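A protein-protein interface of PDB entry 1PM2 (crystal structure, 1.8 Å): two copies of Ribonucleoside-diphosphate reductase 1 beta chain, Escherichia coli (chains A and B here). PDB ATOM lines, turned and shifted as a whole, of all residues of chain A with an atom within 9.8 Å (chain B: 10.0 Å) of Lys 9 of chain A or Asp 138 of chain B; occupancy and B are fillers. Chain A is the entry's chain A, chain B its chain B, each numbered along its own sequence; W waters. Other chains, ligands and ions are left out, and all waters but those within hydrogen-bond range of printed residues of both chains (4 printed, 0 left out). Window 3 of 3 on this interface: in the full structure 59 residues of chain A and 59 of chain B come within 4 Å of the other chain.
No position is printed for both chains.
Of the printed residues of chain B, Lys 9 of chain A touches Asp 138 (3.4 Å), Val 141 (3.96 Å) and Thr 142 (3.7 Å).
Printed residues of chain A within 4 Å of Asp 138 of chain B: Lys 9.
Thr 8 of chain A touches just one residue of chain B: Val 141 (3.9 Å).
No residue of chain B comes within 4 Å of Asn 10 of chain A.
Val 141 of chain B touches just these residues of chain A: Gln 7 (3.5 Å), Thr 8 (3.9 Å), Lys 9 (3.96 Å) and Asn 24 (3.7 Å).
Of the printed residues of chain A, Ser 134 of chain B touches Arg 27.
Printed residues of chain B within 4 Å of Asn 24 of chain A: Val 141 (3.7 Å).
Printed residues of chain B within 4 Å of Arg 27 of chain A: Ser 134 and Phe 137.
Of the printed residues of chain B, Asp 29 of chain A touches Pro 133 and Phe 137.
Of the printed residues of chain B, Phe 5 of chain A touches Leu 82 (3.2 Å) and Gln 147 (3.5 Å).
The nearest residue of chain A that does not touch Asp 138 of chain B is Arg 27 of chain A (4.3 Å).
Water W3 lies within hydrogen-bond range of OD1 of Asp 138 of chain B (2.7 Å) and O of Asn 10 of chain A (2.9 Å).
Water W2 bridges the side-chain amide oxygen (OE1) of Gln 30 of chain A and the side-chain hydroxyl (OG) of Ser 134 of chain B.
Water W4 bridges the side-chain carboxylate of Asp 138 of chain B (3.0 Å) and the guanidinium group of Arg 27 of chain A (3.0 Å).
Water W1 lies within hydrogen-bond range of NH1 of Arg 27 of chain A and OD1 of Asp 138 of chain B.
NH2 of Arg 27 of chain A is in hydrogen-bond range of OG of Ser 134 of chain B, 3.0 Å away.
The side-chain amide nitrogen (NE2) of Gln 21 of chain A is in hydrogen-bond range of the backbone carbonyl oxygen (O) of Thr 8 of chain A (3.0 Å).
The side-chain amide oxygen (OD1) of Asn 10 of chain A is in hydrogen-bond range of the side-chain amide nitrogen (ND2) of Asn 24 of chain A (3.4 Å).
NE2 of Gln 12 of chain A is in hydrogen-bond range of O of Val 25 of chain A, at 3.0 Å.
The side-chain amide nitrogen (ND2) of Asn 24 of chain A lies close to the side-chain amide nitrogen (NE2) of Gln 21 of chain A, 3.3 Å away.
The guanidinium group of Arg 27 of chain A is in salt-bridge range of the side-chain carboxylate of Asp 29 of chain A.
The side-chain amide nitrogen (NE2) of Gln 147 of chain B sits at hydrogen-bond distance from the backbone carbonyl oxygen (O) of Ile 140 of chain B, at 2.8 Å.
Among the printed residues, pairs that only touch across the chains: Phe 5 of chain A with Leu 82 of chain B, Lys 9 of chain A with Asp 138 of chain B, Asp 29 of chain A with Phe 137 of chain B, Phe 5 of chain A with Gln 147 of chain B, Arg 27 of chain A with Phe 137 of chain B, Gln 7 of chain A with Val 141 of chain B, Asp 29 of chain A with Pro 133 of chain B, Lys 9 of chain A with Thr 142 of chain B, Asn 24 of chain A with Val 141 of chain B, Val 25 of chain A with Phe 137 of chain B, Thr 8 of chain A with Val 141 of chain B and Lys 9 of chain A with Val 141 of chain B.
Hydrophobic or aromatic side chains of chain B that line the printed part of chain A: Leu 82, Pro 133, Phe 137 and Val 141.
Of the 18 printed residues of chain A, 8 touch a printed residue of chain B.
Among the printed residues, no Asp or Glu carboxylate lies within 4 Å of a Lys or Arg side-chain nitrogen of the other chain.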
ATOM      1  N   PHE A   5       8.895   7.591 -13.118  1.00  0.00           N
ATOM      2  CA  PHE A   5       9.445   8.746 -13.814  1.00  0.00           C
ATOM      3  C   PHE A   5       8.350   9.532 -14.522  1.00  0.00           C
ATOM      4  O   PHE A   5       8.043   9.276 -15.688  1.00  0.00           O
ATOM      5  CB  PHE A   5      10.526   8.359 -14.834  1.00  0.00           C
ATOM      6  CG  PHE A   5      11.381   9.526 -15.260  1.00  0.00           C
ATOM      7  CD1 PHE A   5      12.483   9.906 -14.504  1.00  0.00           C
ATOM      8  CD2 PHE A   5      11.035  10.297 -16.368  1.00  0.00           C
ATOM      9  CE1 PHE A   5      13.228  11.038 -14.836  1.00  0.00           C
ATOM     10  CE2 PHE A   5      11.776  11.437 -16.710  1.00  0.00           C
ATOM     11  CZ  PHE A   5      12.871  11.806 -15.941  1.00  0.00           C
ATOM     12  N   SER A   6       7.761  10.483 -13.804  1.00  0.00           N
ATOM     13  CA  SER A   6       6.704  11.326 -14.356  1.00  0.00           C
ATOM     14  C   SER A   6       7.256  12.119 -15.539  1.00  0.00           C
ATOM     15  O   SER A   6       8.309  12.748 -15.441  1.00  0.00           O
ATOM     16  CB  SER A   6       6.169  12.273 -13.278  1.00  0.00           C
ATOM     17  OG  SER A   6       7.222  12.942 -12.606  1.00  0.00           O
ATOM     18  N   GLN A   7       6.532  12.089 -16.655  1.00  0.00           N
ATOM     19  CA  GLN A   7       6.963  12.765 -17.872  1.00  0.00           C
ATOM     20  C   GLN A   7       6.664  14.258 -17.933  1.00  0.00           C
ATOM     21  O   GLN A   7       7.080  14.932 -18.873  1.00  0.00           O
ATOM     22  CB  GLN A   7       6.354  12.071 -19.085  1.00  0.00           C
ATOM     23  N   THR A   8       5.941  14.773 -16.945  1.00  0.00           N
ATOM     24  CA  THR A   8       5.603  16.193 -16.916  1.00  0.00           C
ATOM     25  C   THR A   8       6.769  17.020 -16.391  1.00  0.00           C
ATOM     26  O   THR A   8       7.316  16.734 -15.327  1.00  0.00           O
ATOM     27  CB  THR A   8       4.377  16.465 -16.016  1.00  0.00           C
ATOM     28  OG1 THR A   8       3.246  15.737 -16.509  1.00  0.00           O
ATOM     29  CG2 THR A   8       4.047  17.951 -16.000  1.00  0.00           C
ATOM     30  N   LYS A   9       7.154  18.043 -17.147  1.00  0.00           N
ATOM     31  CA  LYS A   9       8.242  18.921 -16.739  1.00  0.00           C
ATOM     32  C   LYS A   9       7.672  19.839 -15.665  1.00  0.00           C
ATOM     33  O   LYS A   9       6.942  20.784 -15.969  1.00  0.00           O
ATOM     34  CB  LYS A   9       8.730  19.736 -17.938  1.00  0.00           C
ATOM     35  CG  LYS A   9       9.831  20.732 -17.632  1.00  0.00           C
ATOM     36  CD  LYS A   9      10.290  21.426 -18.907  1.00  0.00           C
ATOM     37  CE  LYS A   9      11.239  22.573 -18.611  1.00  0.00           C
ATOM     38  NZ  LYS A   9      10.571  23.657 -17.837  1.00  0.00           N
ATOM     39  N   ASN A  10       7.994  19.556 -14.407  1.00  0.00           N
ATOM     40  CA  ASN A  10       7.473  20.358 -13.305  1.00  0.00           C
ATOM     41  C   ASN A  10       8.549  21.073 -12.500  1.00  0.00           C
ATOM     42  O   ASN A  10       9.710  20.662 -12.486  1.00  0.00           O
ATOM     43  CB  ASN A  10       6.635  19.473 -12.374  1.00  0.00           C
ATOM     44  CG  ASN A  10       7.479  18.492 -11.575  1.00  0.00           C
ATOM     45  OD1 ASN A  10       8.335  17.801 -12.124  1.00  0.00           O
ATOM     46  ND2 ASN A  10       7.228  18.422 -10.269  1.00  0.00           N
ATOM     47  N   ASP A  11       8.154  22.157 -11.837  1.00  0.00           N
ATOM     48  CA  ASP A  11       9.075  22.923 -11.006  1.00  0.00           C
ATOM     49  C   ASP A  11       9.102  22.223  -9.651  1.00  0.00           C
ATOM     50  O   ASP A  11       8.139  22.295  -8.884  1.00  0.00           O
ATOM     51  CB  ASP A  11       8.578  24.359 -10.830  1.00  0.00           C
ATOM     52  CG  ASP A  11       9.604  25.248 -10.156  1.00  0.00           C
ATOM     53  OD1 ASP A  11      10.346  24.747  -9.287  1.00  0.00           O
ATOM     54  OD2 ASP A  11       9.664  26.450 -10.485  1.00  0.00           O
ATOM     55  N   GLN A  12      10.205  21.546  -9.362  1.00  0.00           N
ATOM     56  CA  GLN A  12      10.333  20.808  -8.114  1.00  0.00           C
ATOM     57  C   GLN A  12      10.424  21.694  -6.878  1.00  0.00           C
ATOM     58  O   GLN A  12      10.277  21.215  -5.757  1.00  0.00           O
ATOM     59  CB  GLN A  12      11.550  19.889  -8.185  1.00  0.00           C
ATOM     60  CG  GLN A  12      11.496  18.920  -9.354  1.00  0.00           C
ATOM     61  CD  GLN A  12      12.725  18.040  -9.431  1.00  0.00           C
ATOM     62  OE1 GLN A  12      13.852  18.519  -9.310  1.00  0.00           O
ATOM     63  NE2 GLN A  12      12.515  16.745  -9.647  1.00  0.00           N
ATOM     64  N   LEU A  13      10.666  22.984  -7.077  1.00  0.00           N
ATOM     65  CA  LEU A  13      10.753  23.908  -5.951  1.00  0.00           C
ATOM     66  C   LEU A  13       9.360  24.311  -5.465  1.00  0.00           C
ATOM     67  O   LEU A  13       9.200  24.796  -4.341  1.00  0.00           O
ATOM     68  CB  LEU A  13      11.536  25.157  -6.359  1.00  0.00           C
ATOM     69  CG  LEU A  13      12.999  24.944  -6.757  1.00  0.00           C
ATOM     70  CD1 LEU A  13      13.591  26.251  -7.265  1.00  0.00           C
ATOM     71  CD2 LEU A  13      13.784  24.424  -5.560  1.00  0.00           C
ATOM     72  N   GLU A  15       6.597  22.088  -5.557  1.00  0.00           N
ATOM     73  CA  GLU A  15       5.796  20.928  -5.180  1.00  0.00           C
ATOM     74  C   GLU A  15       5.718  20.835  -3.661  1.00  0.00           C
ATOM     75  O   GLU A  15       6.570  21.371  -2.960  1.00  0.00           O
ATOM     76  CB  GLU A  15       6.441  19.638  -5.695  1.00  0.00           C
ATOM     77  CG  GLU A  15       6.453  19.460  -7.206  1.00  0.00           C
ATOM     78  CD  GLU A  15       5.078  19.189  -7.767  1.00  0.00           C
ATOM     79  OE1 GLU A  15       4.263  18.557  -7.062  1.00  0.00           O
ATOM     80  OE2 GLU A  15       4.816  19.588  -8.921  1.00  0.00           O
ATOM     81  N   GLN A  21       3.453  15.785  -7.521  1.00  0.00           N
ATOM     82  CA  GLN A  21       3.827  14.944  -8.656  1.00  0.00           C
ATOM     83  C   GLN A  21       5.005  14.057  -8.252  1.00  0.00           C
ATOM     84  O   GLN A  21       5.933  14.525  -7.600  1.00  0.00           O
ATOM     85  CB  GLN A  21       4.244  15.814  -9.841  1.00  0.00           C
ATOM     86  CG  GLN A  21       4.665  15.027 -11.075  1.00  0.00           C
ATOM     87  CD  GLN A  21       5.146  15.929 -12.194  1.00  0.00           C
ATOM     88  OE1 GLN A  21       4.540  16.965 -12.474  1.00  0.00           O
ATOM     89  NE2 GLN A  21       6.233  15.536 -12.850  1.00  0.00           N
ATOM     90  N   PRO A  22       4.975  12.762  -8.617  1.00  0.00           N
ATOM     91  CA  PRO A  22       6.108  11.911  -8.238  1.00  0.00           C
ATOM     92  C   PRO A  22       7.393  12.534  -8.785  1.00  0.00           C
ATOM     93  O   PRO A  22       7.390  13.135  -9.860  1.00  0.00           O
ATOM     94  CB  PRO A  22       5.769  10.578  -8.896  1.00  0.00           C
ATOM     95  CG  PRO A  22       4.259  10.552  -8.807  1.00  0.00           C
ATOM     96  CD  PRO A  22       3.892  11.965  -9.221  1.00  0.00           C
ATOM     97  N   ASN A  24      10.663  13.121 -10.730  1.00  0.00           N
ATOM     98  CA  ASN A  24      11.250  12.525 -11.924  1.00  0.00           C
ATOM     99  C   ASN A  24      12.771  12.630 -11.862  1.00  0.00           C
ATOM    100  O   ASN A  24      13.440  11.672 -11.474  1.00  0.00           O
ATOM    101  CB  ASN A  24      10.717  13.133 -13.245  1.00  0.00           C
ATOM    102  CG  ASN A  24      10.496  14.637 -13.185  1.00  0.00           C
ATOM    103  OD1 ASN A  24      11.307  15.390 -12.648  1.00  0.00           O
ATOM    104  ND2 ASN A  24       9.389  15.083 -13.781  1.00  0.00           N
ATOM    105  N   VAL A  25      13.325  13.785 -12.214  1.00  0.00           N
ATOM    106  CA  VAL A  25      14.775  13.937 -12.184  1.00  0.00           C
ATOM    107  C   VAL A  25      15.332  14.129 -10.770  1.00  0.00           C
ATOM    108  O   VAL A  25      14.812  14.919  -9.983  1.00  0.00           O
ATOM    109  CB  VAL A  25      15.236  15.123 -13.079  1.00  0.00           C
ATOM    110  CG1 VAL A  25      14.618  16.421 -12.597  1.00  0.00           C
ATOM    111  CG2 VAL A  25      16.757  15.223 -13.067  1.00  0.00           C
ATOM    112  N   ALA A  26      16.382  13.384 -10.443  1.00  0.00           N
ATOM    113  CA  ALA A  26      17.012  13.508  -9.134  1.00  0.00           C
ATOM    114  C   ALA A  26      18.146  14.510  -9.305  1.00  0.00           C
ATOM    115  O   ALA A  26      19.179  14.191  -9.893  1.00  0.00           O
ATOM    116  CB  ALA A  26      17.561  12.154  -8.673  1.00  0.00           C
ATOM    117  N   ARG A  27      17.932  15.727  -8.813  1.00  0.00           N
ATOM    118  CA  ARG A  27      18.922  16.795  -8.904  1.00  0.00           C
ATOM    119  C   ARG A  27      19.193  17.332  -7.506  1.00  0.00           C
ATOM    120  O   ARG A  27      18.294  17.366  -6.663  1.00  0.00           O
ATOM    121  CB  ARG A  27      18.413  17.916  -9.816  1.00  0.00           C
ATOM    122  CG  ARG A  27      17.074  18.503  -9.391  1.00  0.00           C
ATOM    123  CD  ARG A  27      16.543  19.489 -10.432  1.00  0.00           C
ATOM    124  NE  ARG A  27      17.401  20.663 -10.582  1.00  0.00           N
ATOM    125  CZ  ARG A  27      17.125  21.689 -11.384  1.00  0.00           C
ATOM    126  NH1 ARG A  27      16.016  21.685 -12.113  1.00  0.00           N
ATOM    127  NH2 ARG A  27      17.952  22.720 -11.455  1.00  0.00           N
ATOM    128  N   ASP A  29      21.245  20.387  -7.014  1.00  0.00           N
ATOM    129  CA  ASP A  29      21.835  21.715  -7.173  1.00  0.00           C
ATOM    130  C   ASP A  29      20.945  22.786  -6.555  1.00  0.00           C
ATOM    131  O   ASP A  29      21.346  23.944  -6.414  1.00  0.00           O
ATOM    132  CB  ASP A  29      22.016  22.014  -8.659  1.00  0.00           C
ATOM    133  CG  ASP A  29      20.700  22.022  -9.411  1.00  0.00           C
ATOM    134  OD1 ASP A  29      19.907  21.073  -9.235  1.00  0.00           O
ATOM    135  OD2 ASP A  29      20.453  22.972 -10.182  1.00  0.00           O
ATOM    136  N   GLN A  30      19.733  22.389  -6.197  1.00  0.00           N
ATOM    137  CA  GLN A  30      18.762  23.298  -5.605  1.00  0.00           C
ATOM    138  C   GLN A  30      17.762  22.473  -4.823  1.00  0.00           C
ATOM    139  O   GLN A  30      17.649  21.268  -5.026  1.00  0.00           O
ATOM    140  CB  GLN A  30      18.008  24.054  -6.699  1.00  0.00           C
ATOM    141  CG  GLN A  30      17.321  23.121  -7.700  1.00  0.00           C
ATOM    142  CD  GLN A  30      16.321  23.830  -8.589  1.00  0.00           C
ATOM    143  OE1 GLN A  30      16.581  24.926  -9.084  1.00  0.00           O
ATOM    144  NE2 GLN A  30      15.170  23.198  -8.808  1.00  0.00           N
ATOM    145  N   LYS B  78      23.173  13.438 -19.859  1.00  0.00           N
ATOM    146  CA  LYS B  78      21.766  13.574 -19.505  1.00  0.00           C
ATOM    147  C   LYS B  78      21.078  12.210 -19.425  1.00  0.00           C
ATOM    148  O   LYS B  78      20.255  11.976 -18.539  1.00  0.00           O
ATOM    149  CB  LYS B  78      21.059  14.493 -20.506  1.00  0.00           C
ATOM    150  CG  LYS B  78      21.421  15.964 -20.293  1.00  0.00           C
ATOM    151  CD  LYS B  78      20.674  16.903 -21.231  1.00  0.00           C
ATOM    152  CE  LYS B  78      21.216  16.841 -22.640  1.00  0.00           C
ATOM    153  NZ  LYS B  78      20.673  17.967 -23.468  1.00  0.00           N
ATOM    154  N   THR B  81      22.104  10.475 -16.262  1.00  0.00           N
ATOM    155  CA  THR B  81      21.403  11.085 -15.136  1.00  0.00           C
ATOM    156  C   THR B  81      19.960  10.589 -15.059  1.00  0.00           C
ATOM    157  O   THR B  81      19.426  10.363 -13.973  1.00  0.00           O
ATOM    158  CB  THR B  81      21.439  12.619 -15.249  1.00  0.00           C
ATOM    159  OG1 THR B  81      22.802  13.045 -15.363  1.00  0.00           O
ATOM    160  CG2 THR B  81      20.818  13.265 -14.015  1.00  0.00           C
ATOM    161  N   LEU B  82      19.332  10.417 -16.218  1.00  0.00           N
ATOM    162  CA  LEU B  82      17.967   9.913 -16.276  1.00  0.00           C
ATOM    163  C   LEU B  82      17.926   8.505 -15.681  1.00  0.00           C
ATOM    164  O   LEU B  82      17.087   8.204 -14.827  1.00  0.00           O
ATOM    165  CB  LEU B  82      17.486   9.875 -17.735  1.00  0.00           C
ATOM    166  CG  LEU B  82      16.135   9.242 -18.100  1.00  0.00           C
ATOM    167  CD1 LEU B  82      16.155   7.738 -17.873  1.00  0.00           C
ATOM    168  CD2 LEU B  82      15.042   9.887 -17.284  1.00  0.00           C
ATOM    169  N   ILE B 126      27.600  18.312 -13.474  1.00  0.00           N
ATOM    170  CA  ILE B 126      26.819  19.323 -14.174  1.00  0.00           C
ATOM    171  C   ILE B 126      27.021  20.732 -13.628  1.00  0.00           C
ATOM    172  O   ILE B 126      27.230  21.671 -14.394  1.00  0.00           O
ATOM    173  CB  ILE B 126      25.317  18.968 -14.141  1.00  0.00           C
ATOM    174  CG1 ILE B 126      25.078  17.705 -14.973  1.00  0.00           C
ATOM    175  CG2 ILE B 126      24.485  20.124 -14.684  1.00  0.00           C
ATOM    176  CD1 ILE B 126      23.680  17.121 -14.829  1.00  0.00           C
ATOM    177  N   ASP B 132      24.211  27.321 -15.874  1.00  0.00           N
ATOM    178  CA  ASP B 132      22.865  27.118 -15.345  1.00  0.00           C
ATOM    179  C   ASP B 132      22.440  25.658 -15.475  1.00  0.00           C
ATOM    180  O   ASP B 132      21.907  25.241 -16.502  1.00  0.00           O
ATOM    181  CB  ASP B 132      21.859  28.009 -16.080  1.00  0.00           C
ATOM    182  CG  ASP B 132      20.453  27.889 -15.516  1.00  0.00           C
ATOM    183  OD1 ASP B 132      19.536  28.547 -16.051  1.00  0.00           O
ATOM    184  OD2 ASP B 132      20.262  27.136 -14.535  1.00  0.00           O
ATOM    185  N   PRO B 133      22.671  24.862 -14.421  1.00  0.00           N
ATOM    186  CA  PRO B 133      22.316  23.440 -14.404  1.00  0.00           C
ATOM    187  C   PRO B 133      20.861  23.156 -14.770  1.00  0.00           C
ATOM    188  O   PRO B 133      20.553  22.103 -15.326  1.00  0.00           O
ATOM    189  CB  PRO B 133      22.635  23.029 -12.970  1.00  0.00           C
ATOM    190  CG  PRO B 133      23.801  23.903 -12.632  1.00  0.00           C
ATOM    191  CD  PRO B 133      23.354  25.243 -13.173  1.00  0.00           C
ATOM    192  N   SER B 134      19.967  24.092 -14.457  1.00  0.00           N
ATOM    193  CA  SER B 134      18.545  23.916 -14.745  1.00  0.00           C
ATOM    194  C   SER B 134      18.256  23.589 -16.205  1.00  0.00           C
ATOM    195  O   SER B 134      17.327  22.840 -16.505  1.00  0.00           O
ATOM    196  CB  SER B 134      17.759  25.162 -14.334  1.00  0.00           C
ATOM    197  OG  SER B 134      17.755  25.308 -12.927  1.00  0.00           O
ATOM    198  N   VAL B 135      19.045  24.154 -17.109  1.00  0.00           N
ATOM    199  CA  VAL B 135      18.856  23.896 -18.530  1.00  0.00           C
ATOM    200  C   VAL B 135      19.038  22.407 -18.801  1.00  0.00           C
ATOM    201  O   VAL B 135      18.226  21.783 -19.482  1.00  0.00           O
ATOM    202  CB  VAL B 135      19.871  24.687 -19.381  1.00  0.00           C
ATOM    203  CG1 VAL B 135      19.691  24.349 -20.856  1.00  0.00           C
ATOM    204  CG2 VAL B 135      19.684  26.181 -19.155  1.00  0.00           C
ATOM    205  N   VAL B 136      20.107  21.843 -18.245  1.00  0.00           N
ATOM    206  CA  VAL B 136      20.409  20.426 -18.418  1.00  0.00           C
ATOM    207  C   VAL B 136      19.347  19.531 -17.775  1.00  0.00           C
ATOM    208  O   VAL B 136      18.825  18.616 -18.408  1.00  0.00           O
ATOM    209  CB  VAL B 136      21.790  20.080 -17.800  1.00  0.00           C
ATOM    210  CG1 VAL B 136      22.070  18.592 -17.944  1.00  0.00           C
ATOM    211  CG2 VAL B 136      22.880  20.889 -18.478  1.00  0.00           C
ATOM    212  N   PHE B 137      19.026  19.801 -16.515  1.00  0.00           N
ATOM    213  CA  PHE B 137      18.045  18.992 -15.805  1.00  0.00           C
ATOM    214  C   PHE B 137      16.653  18.971 -16.426  1.00  0.00           C
ATOM    215  O   PHE B 137      16.030  17.910 -16.508  1.00  0.00           O
ATOM    216  CB  PHE B 137      17.974  19.427 -14.340  1.00  0.00           C
ATOM    217  CG  PHE B 137      19.181  19.023 -13.540  1.00  0.00           C
ATOM    218  CD1 PHE B 137      19.566  17.686 -13.475  1.00  0.00           C
ATOM    219  CD2 PHE B 137      19.937  19.970 -12.860  1.00  0.00           C
ATOM    220  CE1 PHE B 137      20.688  17.299 -12.744  1.00  0.00           C
ATOM    221  CE2 PHE B 137      21.061  19.592 -12.126  1.00  0.00           C
ATOM    222  CZ  PHE B 137      21.436  18.257 -12.069  1.00  0.00           C
ATOM    223  N   ASP B 138      16.160  20.121 -16.873  1.00  0.00           N
ATOM    224  CA  ASP B 138      14.835  20.158 -17.485  1.00  0.00           C
ATOM    225  C   ASP B 138      14.793  19.375 -18.793  1.00  0.00           C
ATOM    226  O   ASP B 138      13.800  18.709 -19.095  1.00  0.00           O
ATOM    227  CB  ASP B 138      14.386  21.599 -17.748  1.00  0.00           C
ATOM    228  CG  ASP B 138      14.036  22.344 -16.474  1.00  0.00           C
ATOM    229  OD1 ASP B 138      13.448  21.720 -15.562  1.00  0.00           O
ATOM    230  OD2 ASP B 138      14.334  23.555 -16.392  1.00  0.00           O
ATOM    231  N   ASP B 139      15.871  19.442 -19.565  1.00  0.00           N
ATOM    232  CA  ASP B 139      15.907  18.735 -20.838  1.00  0.00           C
ATOM    233  C   ASP B 139      15.881  17.220 -20.660  1.00  0.00           C
ATOM    234  O   ASP B 139      15.490  16.489 -21.565  1.00  0.00           O
ATOM    235  CB  ASP B 139      17.142  19.137 -21.642  1.00  0.00           C
ATOM    236  CG  ASP B 139      17.106  18.593 -23.054  1.00  0.00           C
ATOM    237  OD1 ASP B 139      16.152  18.923 -23.790  1.00  0.00           O
ATOM    238  OD2 ASP B 139      18.022  17.830 -23.427  1.00  0.00           O
ATOM    239  N   ILE B 140      16.296  16.746 -19.492  1.00  0.00           N
ATOM    240  CA  ILE B 140      16.300  15.314 -19.227  1.00  0.00           C
ATOM    241  C   ILE B 140      14.874  14.769 -19.210  1.00  0.00           C
ATOM    242  O   ILE B 140      14.612  13.659 -19.677  1.00  0.00           O
ATOM    243  CB  ILE B 140      16.979  15.001 -17.873  1.00  0.00           C
ATOM    244  CG1 ILE B 140      18.474  15.319 -17.960  1.00  0.00           C
ATOM    245  CG2 ILE B 140      16.765  13.536 -17.504  1.00  0.00           C
ATOM    246  CD1 ILE B 140      19.217  15.164 -16.647  1.00  0.00           C
ATOM    247  N   VAL B 141      13.948  15.558 -18.682  1.00  0.00           N
ATOM    248  CA  VAL B 141      12.560  15.138 -18.594  1.00  0.00           C
ATOM    249  C   VAL B 141      11.815  15.144 -19.928  1.00  0.00           C
ATOM    250  O   VAL B 141      11.057  14.221 -20.222  1.00  0.00           O
ATOM    251  CB  VAL B 141      11.778  16.030 -17.600  1.00  0.00           C
ATOM    252  CG1 VAL B 141      10.305  15.662 -17.615  1.00  0.00           C
ATOM    253  CG2 VAL B 141      12.350  15.870 -16.200  1.00  0.00           C
ATOM    254  N   THR B 142      12.046  16.175 -20.735  1.00  0.00           N
ATOM    255  CA  THR B 142      11.354  16.327 -22.013  1.00  0.00           C
ATOM    256  C   THR B 142      12.098  15.930 -23.286  1.00  0.00           C
ATOM    257  O   THR B 142      11.475  15.810 -24.344  1.00  0.00           O
ATOM    258  CB  THR B 142      10.907  17.782 -22.207  1.00  0.00           C
ATOM    259  OG1 THR B 142      12.062  18.631 -22.183  1.00  0.00           O
ATOM    260  CG2 THR B 142       9.946  18.202 -21.106  1.00  0.00           C
ATOM    261  N   ASN B 143      13.411  15.746 -23.203  1.00  0.00           N
ATOM    262  CA  ASN B 143      14.189  15.386 -24.390  1.00  0.00           C
ATOM    263  C   ASN B 143      13.575  14.186 -25.104  1.00  0.00           C
ATOM    264  O   ASN B 143      13.569  13.072 -24.582  1.00  0.00           O
ATOM    265  CB  ASN B 143      15.642  15.088 -24.007  1.00  0.00           C
ATOM    266  CG  ASN B 143      16.524  14.855 -25.217  1.00  0.00           C
ATOM    267  OD1 ASN B 143      16.325  13.904 -25.970  1.00  0.00           O
ATOM    268  ND2 ASN B 143      17.501  15.731 -25.411  1.00  0.00           N
ATOM    269  N   GLU B 144      13.061  14.422 -26.306  1.00  0.00           N
ATOM    270  CA  GLU B 144      12.416  13.371 -27.085  1.00  0.00           C
ATOM    271  C   GLU B 144      13.285  12.158 -27.375  1.00  0.00           C
ATOM    272  O   GLU B 144      12.824  11.024 -27.261  1.00  0.00           O
ATOM    273  CB  GLU B 144      11.887  13.942 -28.405  1.00  0.00           C
ATOM    274  CG  GLU B 144      10.706  14.882 -28.233  1.00  0.00           C
ATOM    275  CD  GLU B 144      10.161  15.386 -29.556  1.00  0.00           C
ATOM    276  OE1 GLU B 144       9.130  16.094 -29.540  1.00  0.00           O
ATOM    277  OE2 GLU B 144      10.763  15.077 -30.608  1.00  0.00           O
ATOM    278  N   ILE B 146      15.922  11.153 -25.697  1.00  0.00           N
ATOM    279  CA  ILE B 146      16.270  10.473 -24.457  1.00  0.00           C
ATOM    280  C   ILE B 146      15.020   9.817 -23.890  1.00  0.00           C
ATOM    281  O   ILE B 146      15.011   8.620 -23.601  1.00  0.00           O
ATOM    282  CB  ILE B 146      16.837  11.459 -23.411  1.00  0.00           C
ATOM    283  CG1 ILE B 146      18.194  11.988 -23.880  1.00  0.00           C
ATOM    284  CG2 ILE B 146      16.966  10.772 -22.060  1.00  0.00           C
ATOM    285  CD1 ILE B 146      18.838  12.974 -22.926  1.00  0.00           C
ATOM    286  N   GLN B 147      13.965  10.613 -23.747  1.00  0.00           N
ATOM    287  CA  GLN B 147      12.698  10.136 -23.209  1.00  0.00           C
ATOM    288  C   GLN B 147      11.970   9.202 -24.152  1.00  0.00           C
ATOM    289  O   GLN B 147      10.926   9.545 -24.709  1.00  0.00           O
ATOM    290  CB  GLN B 147      11.790  11.314 -22.860  1.00  0.00           C
ATOM    291  CG  GLN B 147      12.199  12.028 -21.592  1.00  0.00           C
ATOM    292  CD  GLN B 147      12.284  11.083 -20.412  1.00  0.00           C
ATOM    293  OE1 GLN B 147      11.338  10.353 -20.116  1.00  0.00           O
ATOM    294  NE2 GLN B 147      13.422  11.090 -19.732  1.00  0.00           N
HETATM  295  O   HOH W   1      13.726  19.771 -12.812  1.00  0.00           O
HETATM  296  O   HOH W   2      15.500  26.450 -11.004  1.00  0.00           O
HETATM  297  O   HOH W   3      11.400  22.439 -14.031  1.00  0.00           O
HETATM  298  O   HOH W   4      14.545  23.922 -13.472  1.00  0.00           O
